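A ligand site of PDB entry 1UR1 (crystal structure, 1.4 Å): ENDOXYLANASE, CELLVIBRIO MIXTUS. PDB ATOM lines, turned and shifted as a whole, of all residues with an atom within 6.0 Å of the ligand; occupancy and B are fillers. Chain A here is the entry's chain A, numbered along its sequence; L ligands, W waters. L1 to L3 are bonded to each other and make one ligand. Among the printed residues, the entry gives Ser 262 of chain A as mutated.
Water W6 bridges an oxygen (O3) of LG3 L3 (2.6 Å) and the side-chain amide nitrogen of Asn 42 (3.2 Å). Water W5 lies within hydrogen-bond range of O4 of LG3 L3 and O of Ser 335. Water W4 lies within hydrogen-bond range of the side-chain hydroxyl of Ser 262 (2.6 Å), an oxygen (O2) of LIG L1 (2.8 Å) and the side-chain amide nitrogen of Asn 198 (3.5 Å). Water W1 lies within hydrogen-bond range of an oxygen (O5) of LIG L1 (3.0 Å) and the side-chain carboxylate of Glu 157 (3.1 Å). Water W3 lies within hydrogen-bond range of the side-chain carboxylate (OE1) of Glu 67 (2.5 Å), the backbone carbonyl oxygen (O) of Ala 334 (2.6 Å), the side-chain amide nitrogen (ND2) of Asn 42 (3.1 Å) and an oxygen (O4) of LG3 L3 (3.3 Å).
CH2 of Trp 108 touches O3 of LIG L1, 3.5 Å away. OE2 of Glu 157 touches C1 of LIG L1, 3.8 Å away. O of Ala 334 touches O4 of LG3 L3, 3.7 Å away. CB of Trp 336 touches O1 of LG2 L2 (3.4 Å). Hydrophobic or aromatic side chains that line the ligand: His 104, Trp 108, His 233, Trp 328 and Trp 336. 14 residues have an atom within 4 Å of the ligand: Glu 67, Asn 68, Lys 71, His 104, Trp 108, Gln 111, Asn 156, Glu 157, Gln 231, His 233, Ser 262, Trp 328, Ala 334 and Trp 336. The nearest printed residue that does not touch the ligand is Asn 198 (4.1 Å).
O of Glu 67 is in hydrogen-bond range of NZ of Lys 71 (2.9 Å). A ring nitrogen (ND1) of His 104 sits at hydrogen-bond distance from the side-chain carboxylate (OD2) of Asp 153 (2.7 Å). OE1 of Gln 111 is in hydrogen-bond range of NZ of Lys 71 (2.9 Å). The side-chain amide nitrogen (NE2) of Gln 231 sits at hydrogen-bond distance from the side-chain carboxylate (OE2) of Glu 157. OD1 of Asn 68 is in hydrogen-bond range of NE2 of Gln 111. The side-chain hydroxyl (OG1) of Thr 261 lies within hydrogen-bond range of the side-chain hydroxyl (OG) of Ser 262 (2.9 Å). The indole nitrogen (NE1) of Trp 108 is in hydrogen-bond range of the side-chain carboxylate (OE1) of Glu 157, 2.9 Å away. N of Glu 157 lies within hydrogen-bond range of O of Asn 198, at 2.9 Å.
OE2 of Glu 67 sits at hydrogen-bond distance from O1 of LG2 L2. A ring nitrogen (NE2) of His 104 sits at hydrogen-bond distance from an oxygen (O3) of LIG L1 (2.8 Å). An oxygen (O3) of LIG L1 is in hydrogen-bond range of the side-chain amino group of Lys 71 (2.8 Å). A ring nitrogen (NE2) of His 233 sits at hydrogen-bond distance from an oxygen (O1) of LIG L1, 2.8 Å away. NE1 of Trp 328 is in hydrogen-bond range of O1 of LG2 L2 (2.9 Å). The side-chain amide nitrogen (ND2) of Asn 156 lies within hydrogen-bond range of an oxygen (O2) of LIG L1, 3.0 Å away. An oxygen (O1) of LIG L1 lies within hydrogen-bond range of the side-chain amide oxygen (OE1) of Gln 231 (3.0 Å). The side-chain amide nitrogen (ND2) of Asn 68 sits at hydrogen-bond distance from an oxygen (O2) of LG2 L2 (3.1 Å). The side-chain amide oxygen (OE1) of Gln 111 lies close to an oxygen (O4) of LG2 L2, at 3.1 Å. O1 of LIG L1 lies within hydrogen-bond range of OG of Ser 262, at 3.4 Å.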
ATOM      1  N   ASN A  42       3.523 -31.730  33.693  1.00  0.00           N
ATOM      2  CA  ASN A  42       2.388 -31.298  34.482  1.00  0.00           C
ATOM      3  C   ASN A  42       2.823 -31.091  35.945  1.00  0.00           C
ATOM      4  O   ASN A  42       3.953 -31.359  36.342  1.00  0.00           O
ATOM      5  CB  ASN A  42       1.247 -32.315  34.342  1.00  0.00           C
ATOM      6  CG  ASN A  42       1.554 -33.657  34.939  1.00  0.00           C
ATOM      7  OD1 ASN A  42       2.008 -33.777  36.062  1.00  0.00           O
ATOM      8  ND2 ASN A  42       1.281 -34.726  34.143  1.00  0.00           N
ATOM      9  N   GLU A  67       3.560 -27.500  31.641  1.00  0.00           N
ATOM     10  CA  GLU A  67       2.414 -27.730  30.771  1.00  0.00           C
ATOM     11  C   GLU A  67       1.293 -26.711  30.956  1.00  0.00           C
ATOM     12  O   GLU A  67       0.598 -26.341  30.001  1.00  0.00           O
ATOM     13  CB  GLU A  67       1.883 -29.170  30.997  1.00  0.00           C
ATOM     14  CG  GLU A  67       0.894 -29.595  29.942  1.00  0.00           C
ATOM     15  CD  GLU A  67       0.461 -31.041  30.074  1.00  0.00           C
ATOM     16  OE1 GLU A  67       1.090 -31.813  30.827  1.00  0.00           O
ATOM     17  OE2 GLU A  67      -0.498 -31.421  29.359  1.00  0.00           O
ATOM     18  N   ASN A  68       1.072 -26.313  32.212  1.00  0.00           N
ATOM     19  CA  ASN A  68      -0.008 -25.351  32.536  1.00  0.00           C
ATOM     20  C   ASN A  68       0.285 -24.284  33.593  1.00  0.00           C
ATOM     21  O   ASN A  68      -0.376 -23.250  33.618  1.00  0.00           O
ATOM     22  CB  ASN A  68      -1.264 -26.085  33.031  1.00  0.00           C
ATOM     23  CG  ASN A  68      -1.962 -26.861  31.918  1.00  0.00           C
ATOM     24  OD1 ASN A  68      -2.442 -26.253  30.947  1.00  0.00           O
ATOM     25  ND2 ASN A  68      -2.046 -28.194  32.066  1.00  0.00           N
ATOM     26  N   LYS A  71       0.668 -20.415  32.969  1.00  0.00           N
ATOM     27  CA  LYS A  71      -0.347 -19.730  32.210  1.00  0.00           C
ATOM     28  C   LYS A  71      -1.092 -18.754  33.123  1.00  0.00           C
ATOM     29  O   LYS A  71      -1.358 -19.071  34.292  1.00  0.00           O
ATOM     30  CB  LYS A  71      -1.304 -20.757  31.594  1.00  0.00           C
ATOM     31  CG  LYS A  71      -0.634 -21.586  30.500  1.00  0.00           C
ATOM     32  CD  LYS A  71      -1.531 -22.756  30.081  1.00  0.00           C
ATOM     33  CE  LYS A  71      -0.741 -23.614  29.080  1.00  0.00           C
ATOM     34  NZ  LYS A  71      -1.538 -24.855  28.671  1.00  0.00           N
ATOM     35  N   HIS A 104       6.334 -20.884  29.777  1.00  0.00           N
ATOM     36  CA  HIS A 104       5.177 -21.014  28.885  1.00  0.00           C
ATOM     37  C   HIS A 104       3.949 -20.556  29.642  1.00  0.00           C
ATOM     38  O   HIS A 104       3.607 -21.172  30.630  1.00  0.00           O
ATOM     39  CB  HIS A 104       5.079 -22.475  28.433  1.00  0.00           C
ATOM     40  CG  HIS A 104       3.899 -22.754  27.550  1.00  0.00           C
ATOM     41  ND1 HIS A 104       3.847 -22.351  26.233  1.00  0.00           N
ATOM     42  CD2 HIS A 104       2.733 -23.405  27.792  1.00  0.00           C
ATOM     43  CE1 HIS A 104       2.690 -22.741  25.714  1.00  0.00           C
ATOM     44  NE2 HIS A 104       1.981 -23.353  26.640  1.00  0.00           N
ATOM     45  N   THR A 105       3.250 -19.488  29.222  1.00  0.00           N
ATOM     46  CA  THR A 105       3.551 -18.526  28.166  1.00  0.00           C
ATOM     47  C   THR A 105       3.064 -17.180  28.670  1.00  0.00           C
ATOM     48  O   THR A 105       2.055 -17.136  29.417  1.00  0.00           O
ATOM     49  CB  THR A 105       2.841 -18.938  26.816  1.00  0.00           C
ATOM     50  OG1 THR A 105       2.950 -17.863  25.878  1.00  0.00           O
ATOM     51  CG2 THR A 105       1.398 -19.177  26.986  1.00  0.00           C
ATOM     52  N   TRP A 108      -1.147 -14.874  25.823  1.00  0.00           N
ATOM     53  CA  TRP A 108      -1.906 -15.851  25.043  1.00  0.00           C
ATOM     54  C   TRP A 108      -3.385 -15.618  25.298  1.00  0.00           C
ATOM     55  O   TRP A 108      -3.760 -15.145  26.355  1.00  0.00           O
ATOM     56  CB  TRP A 108      -1.517 -17.230  25.509  1.00  0.00           C
ATOM     57  CG  TRP A 108      -2.070 -18.417  24.730  1.00  0.00           C
ATOM     58  CD1 TRP A 108      -2.359 -18.479  23.384  1.00  0.00           C
ATOM     59  CD2 TRP A 108      -2.328 -19.715  25.253  1.00  0.00           C
ATOM     60  NE1 TRP A 108      -2.796 -19.747  23.055  1.00  0.00           N
ATOM     61  CE2 TRP A 108      -2.751 -20.527  24.180  1.00  0.00           C
ATOM     62  CE3 TRP A 108      -2.217 -20.282  26.522  1.00  0.00           C
ATOM     63  CZ2 TRP A 108      -3.074 -21.874  24.352  1.00  0.00           C
ATOM     64  CZ3 TRP A 108      -2.564 -21.555  26.709  1.00  0.00           C
ATOM     65  CH2 TRP A 108      -2.964 -22.375  25.622  1.00  0.00           C
ATOM     66  N   GLN A 111      -6.773 -19.888  28.388  1.00  0.00           N
ATOM     67  CA  GLN A 111      -6.450 -20.101  29.802  1.00  0.00           C
ATOM     68  C   GLN A 111      -6.046 -18.783  30.491  1.00  0.00           C
ATOM     69  O   GLN A 111      -5.009 -18.687  31.152  1.00  0.00           O
ATOM     70  CB  GLN A 111      -5.370 -21.187  29.960  1.00  0.00           C
ATOM     71  CG  GLN A 111      -5.947 -22.595  29.654  1.00  0.00           C
ATOM     72  CD  GLN A 111      -4.901 -23.660  29.664  1.00  0.00           C
ATOM     73  OE1 GLN A 111      -4.249 -23.878  28.643  1.00  0.00           O
ATOM     74  NE2 GLN A 111      -4.700 -24.291  30.803  1.00  0.00           N
ATOM     75  N   ASP A 153       8.276 -18.559  25.860  1.00  0.00           N
ATOM     76  CA  ASP A 153       7.234 -18.334  24.868  1.00  0.00           C
ATOM     77  C   ASP A 153       6.552 -17.027  25.294  1.00  0.00           C
ATOM     78  O   ASP A 153       5.723 -17.009  26.207  1.00  0.00           O
ATOM     79  CB  ASP A 153       6.157 -19.421  24.886  1.00  0.00           C
ATOM     80  CG  ASP A 153       6.607 -20.721  24.350  1.00  0.00           C
ATOM     81  OD1 ASP A 153       7.557 -20.782  23.540  1.00  0.00           O
ATOM     82  OD2 ASP A 153       6.012 -21.762  24.701  1.00  0.00           O
ATOM     83  N   ASN A 156       1.961 -16.610  22.237  1.00  0.00           N
ATOM     84  CA  ASN A 156       1.496 -17.933  21.728  1.00  0.00           C
ATOM     85  C   ASN A 156       0.270 -17.683  20.832  1.00  0.00           C
ATOM     86  O   ASN A 156      -0.647 -16.963  21.206  1.00  0.00           O
ATOM     87  CB  ASN A 156       1.124 -18.823  22.941  1.00  0.00           C
ATOM     88  CG  ASN A 156       1.169 -20.328  22.663  1.00  0.00           C
ATOM     89  OD1 ASN A 156       1.977 -20.797  21.879  1.00  0.00           O
ATOM     90  ND2 ASN A 156       0.296 -21.110  23.350  1.00  0.00           N
ATOM     91  N   GLU A 157       0.297 -18.235  19.633  1.00  0.00           N
ATOM     92  CA  GLU A 157      -0.918 -18.408  18.815  1.00  0.00           C
ATOM     93  C   GLU A 157      -1.633 -17.113  18.417  1.00  0.00           C
ATOM     94  O   GLU A 157      -2.845 -16.985  18.622  1.00  0.00           O
ATOM     95  CB  GLU A 157      -1.872 -19.387  19.501  1.00  0.00           C
ATOM     96  CG  GLU A 157      -1.270 -20.746  19.743  1.00  0.00           C
ATOM     97  CD  GLU A 157      -2.162 -21.711  20.440  1.00  0.00           C
ATOM     98  OE1 GLU A 157      -3.349 -21.379  20.754  1.00  0.00           O
ATOM     99  OE2 GLU A 157      -1.695 -22.843  20.706  1.00  0.00           O
ATOM    100  N   ASN A 198       5.458 -18.614  19.409  1.00  0.00           N
ATOM    101  CA  ASN A 198       5.108 -20.030  19.296  1.00  0.00           C
ATOM    102  C   ASN A 198       3.732 -20.182  18.646  1.00  0.00           C
ATOM    103  O   ASN A 198       2.819 -19.433  18.979  1.00  0.00           O
ATOM    104  CB  ASN A 198       5.060 -20.585  20.712  1.00  0.00           C
ATOM    105  CG  ASN A 198       4.999 -22.122  20.820  1.00  0.00           C
ATOM    106  OD1 ASN A 198       5.765 -22.837  20.195  1.00  0.00           O
ATOM    107  ND2 ASN A 198       4.133 -22.614  21.739  1.00  0.00           N
ATOM    108  N   GLN A 231       4.824 -25.684  17.034  1.00  0.00           N
ATOM    109  CA  GLN A 231       4.337 -26.589  18.070  1.00  0.00           C
ATOM    110  C   GLN A 231       4.495 -28.059  17.683  1.00  0.00           C
ATOM    111  O   GLN A 231       4.945 -28.847  18.492  1.00  0.00           O
ATOM    112  CB  GLN A 231       2.891 -26.255  18.423  1.00  0.00           C
ATOM    113  CG  GLN A 231       2.766 -25.011  19.279  1.00  0.00           C
ATOM    114  CD  GLN A 231       1.339 -24.677  19.649  1.00  0.00           C
ATOM    115  OE1 GLN A 231       0.470 -25.544  19.638  1.00  0.00           O
ATOM    116  NE2 GLN A 231       1.087 -23.408  20.030  1.00  0.00           N
ATOM    117  N   HIS A 233       2.042 -30.323  16.718  1.00  0.00           N
ATOM    118  CA  HIS A 233       0.931 -31.221  17.004  1.00  0.00           C
ATOM    119  C   HIS A 233       0.554 -31.825  15.656  1.00  0.00           C
ATOM    120  O   HIS A 233      -0.207 -31.245  14.885  1.00  0.00           O
ATOM    121  CB  HIS A 233      -0.218 -30.472  17.627  1.00  0.00           C
ATOM    122  CG  HIS A 233       0.068 -29.977  19.004  1.00  0.00           C
ATOM    123  ND1 HIS A 233       0.359 -30.820  20.032  1.00  0.00           N
ATOM    124  CD2 HIS A 233       0.063 -28.715  19.522  1.00  0.00           C
ATOM    125  CE1 HIS A 233       0.544 -30.126  21.137  1.00  0.00           C
ATOM    126  NE2 HIS A 233       0.345 -28.850  20.860  1.00  0.00           N
ATOM    127  N   THR A 261       8.185 -27.440  19.733  1.00  0.00           N
ATOM    128  CA  THR A 261       7.911 -27.122  21.128  1.00  0.00           C
ATOM    129  C   THR A 261       6.933 -28.003  21.829  1.00  0.00           C
ATOM    130  O   THR A 261       6.911 -28.015  23.036  1.00  0.00           O
ATOM    131  CB  THR A 261       7.459 -25.714  21.265  1.00  0.00           C
ATOM    132  OG1 THR A 261       6.182 -25.526  20.646  1.00  0.00           O
ATOM    133  CG2 THR A 261       8.389 -24.736  20.581  1.00  0.00           C
ATOM    134  N   SER A 262       6.066 -28.672  21.052  1.00  0.00           N
ATOM    135  CA  SER A 262       4.905 -29.318  21.613  1.00  0.00           C
ATOM    136  C   SER A 262       4.592 -30.597  20.850  1.00  0.00           C
ATOM    137  O   SER A 262       3.447 -30.846  20.561  1.00  0.00           O
ATOM    138  CB  SER A 262       3.679 -28.404  21.549  1.00  0.00           C
ATOM    139  OG  SER A 262       4.024 -27.057  21.923  1.00  0.00           O
ATOM    140  N   TRP A 328       5.117 -32.824  23.970  1.00  0.00           N
ATOM    141  CA  TRP A 328       4.054 -32.251  24.839  1.00  0.00           C
ATOM    142  C   TRP A 328       3.543 -33.316  25.832  1.00  0.00           C
ATOM    143  O   TRP A 328       2.367 -33.709  25.802  1.00  0.00           O
ATOM    144  CB  TRP A 328       2.933 -31.574  24.033  1.00  0.00           C
ATOM    145  CG  TRP A 328       2.260 -30.515  24.857  1.00  0.00           C
ATOM    146  CD1 TRP A 328       0.996 -30.501  25.326  1.00  0.00           C
ATOM    147  CD2 TRP A 328       2.874 -29.308  25.372  1.00  0.00           C
ATOM    148  NE1 TRP A 328       0.785 -29.408  26.129  1.00  0.00           N
ATOM    149  CE2 TRP A 328       1.919 -28.647  26.164  1.00  0.00           C
ATOM    150  CE3 TRP A 328       4.142 -28.726  25.247  1.00  0.00           C
ATOM    151  CZ2 TRP A 328       2.174 -27.449  26.789  1.00  0.00           C
ATOM    152  CZ3 TRP A 328       4.404 -27.521  25.937  1.00  0.00           C
ATOM    153  CH2 TRP A 328       3.420 -26.918  26.687  1.00  0.00           C
ATOM    154  N   ALA A 334      -0.565 -39.299  30.259  1.00  0.00           N
ATOM    155  CA  ALA A 334      -0.714 -37.901  30.647  1.00  0.00           C
ATOM    156  C   ALA A 334      -0.739 -36.972  29.448  1.00  0.00           C
ATOM    157  O   ALA A 334      -0.447 -35.788  29.578  1.00  0.00           O
ATOM    158  CB  ALA A 334       0.432 -37.525  31.574  1.00  0.00           C
ATOM    159  N   SER A 335      -1.146 -37.445  28.262  1.00  0.00           N
ATOM    160  CA  SER A 335      -1.224 -36.598  27.096  1.00  0.00           C
ATOM    161  C   SER A 335      -2.570 -35.859  27.008  1.00  0.00           C
ATOM    162  O   SER A 335      -3.629 -36.445  27.172  1.00  0.00           O
ATOM    163  CB  SER A 335      -1.059 -37.425  25.821  1.00  0.00           C
ATOM    164  OG  SER A 335      -1.297 -36.655  24.693  1.00  0.00           O
ATOM    165  N   TRP A 336      -2.515 -34.581  26.679  1.00  0.00           N
ATOM    166  CA  TRP A 336      -3.712 -33.789  26.474  1.00  0.00           C
ATOM    167  C   TRP A 336      -4.587 -34.319  25.328  1.00  0.00           C
ATOM    168  O   TRP A 336      -5.764 -33.979  25.266  1.00  0.00           O
ATOM    169  CB  TRP A 336      -3.343 -32.305  26.237  1.00  0.00           C
ATOM    170  CG  TRP A 336      -2.822 -31.991  24.858  1.00  0.00           C
ATOM    171  CD1 TRP A 336      -1.729 -32.535  24.232  1.00  0.00           C
ATOM    172  CD2 TRP A 336      -3.368 -31.041  23.958  1.00  0.00           C
ATOM    173  NE1 TRP A 336      -1.613 -31.998  22.976  1.00  0.00           N
ATOM    174  CE2 TRP A 336      -2.579 -31.040  22.800  1.00  0.00           C
ATOM    175  CE3 TRP A 336      -4.439 -30.135  24.020  1.00  0.00           C
ATOM    176  CZ2 TRP A 336      -2.854 -30.227  21.714  1.00  0.00           C
ATOM    177  CZ3 TRP A 336      -4.692 -29.336  22.952  1.00  0.00           C
ATOM    178  CH2 TRP A 336      -3.917 -29.376  21.809  1.00  0.00           C
HETATM  179  C1  LIG L   1      -0.539 -25.882  22.624  1.00  0.00           C
HETATM  180  C2  LIG L   1      -0.412 -24.863  23.750  1.00  0.00           C
HETATM  181  C3  LIG L   1      -0.358 -25.602  25.059  1.00  0.00           C
HETATM  182  C4  LIG L   1      -1.560 -26.513  25.166  1.00  0.00           C
HETATM  183  C5  LIG L   1      -1.552 -27.509  23.991  1.00  0.00           C
HETATM  184  O1  LIG L   1       0.653 -26.597  22.429  1.00  0.00           O
HETATM  185  O2  LIG L   1       0.732 -24.055  23.505  1.00  0.00           O
HETATM  186  O3  LIG L   1      -0.374 -24.703  26.176  1.00  0.00           O
HETATM  187  O4  LIG L   1      -1.493 -27.188  26.396  1.00  0.00           O
HETATM  188  O5  LIG L   1      -1.612 -26.755  22.797  1.00  0.00           O
HETATM  189  C1  LG2 L   2      -2.776 -27.665  26.846  1.00  0.00           C
HETATM  190  C2  LG2 L   2      -2.504 -28.618  27.970  1.00  0.00           C
HETATM  191  C3  LG2 L   2      -3.799 -29.043  28.650  1.00  0.00           C
HETATM  192  C4  LG2 L   2      -4.710 -27.846  28.911  1.00  0.00           C
HETATM  193  C5  LG2 L   2      -4.832 -26.971  27.709  1.00  0.00           C
HETATM  194  O1  LG2 L   2      -1.679 -29.732  27.597  1.00  0.00           O
HETATM  195  O2  LG2 L   2      -3.490 -29.769  29.845  1.00  0.00           O
HETATM  196  O3  LG2 L   2      -5.991 -28.322  29.288  1.00  0.00           O
HETATM  197  O4  LG2 L   2      -3.539 -26.601  27.270  1.00  0.00           O
HETATM  198  O1  LG3 L   3      -7.437 -32.662  31.398  1.00  0.00           O
HETATM  199  C1  LG3 L   3      -6.785 -31.851  32.380  1.00  0.00           C
HETATM  200  C2  LG3 L   3      -5.435 -31.358  31.858  1.00  0.00           C
HETATM  201  O2  LG3 L   3      -5.475 -30.939  30.493  1.00  0.00           O
HETATM  202  C3  LG3 L   3      -4.355 -32.437  31.921  1.00  0.00           C
HETATM  203  O3  LG3 L   3      -3.805 -32.503  33.236  1.00  0.00           O
HETATM  204  C4  LG3 L   3      -3.343 -31.951  30.904  1.00  0.00           C
HETATM  205  O4  LG3 L   3      -2.805 -32.974  30.046  1.00  0.00           O
HETATM  206  C5  LG3 L   3      -4.106 -30.963  30.048  1.00  0.00           C
HETATM  207  O   HOH W   1      -3.698 -24.823  21.897  1.00  0.00           O
HETATM  208  O   HOH W   2      -7.141 -29.769  27.201  1.00  0.00           O
HETATM  209  O   HOH W   3       0.012 -34.012  31.460  1.00  0.00           O
HETATM  210  O   HOH W   4       3.247 -25.324  23.733  1.00  0.00           O
HETATM  211  O   HOH W   5      -4.097 -35.458  30.039  1.00  0.00           O
HETATM  212  O   HOH W   6      -1.816 -34.190  33.603  1.00  0.00           O
HETATM  213  O   HOH W   7      -6.117 -28.077  32.029  1.00  0.00           O
HETATM  214  O   HOH W   8      -8.086 -26.155  29.194  1.00  0.00           O
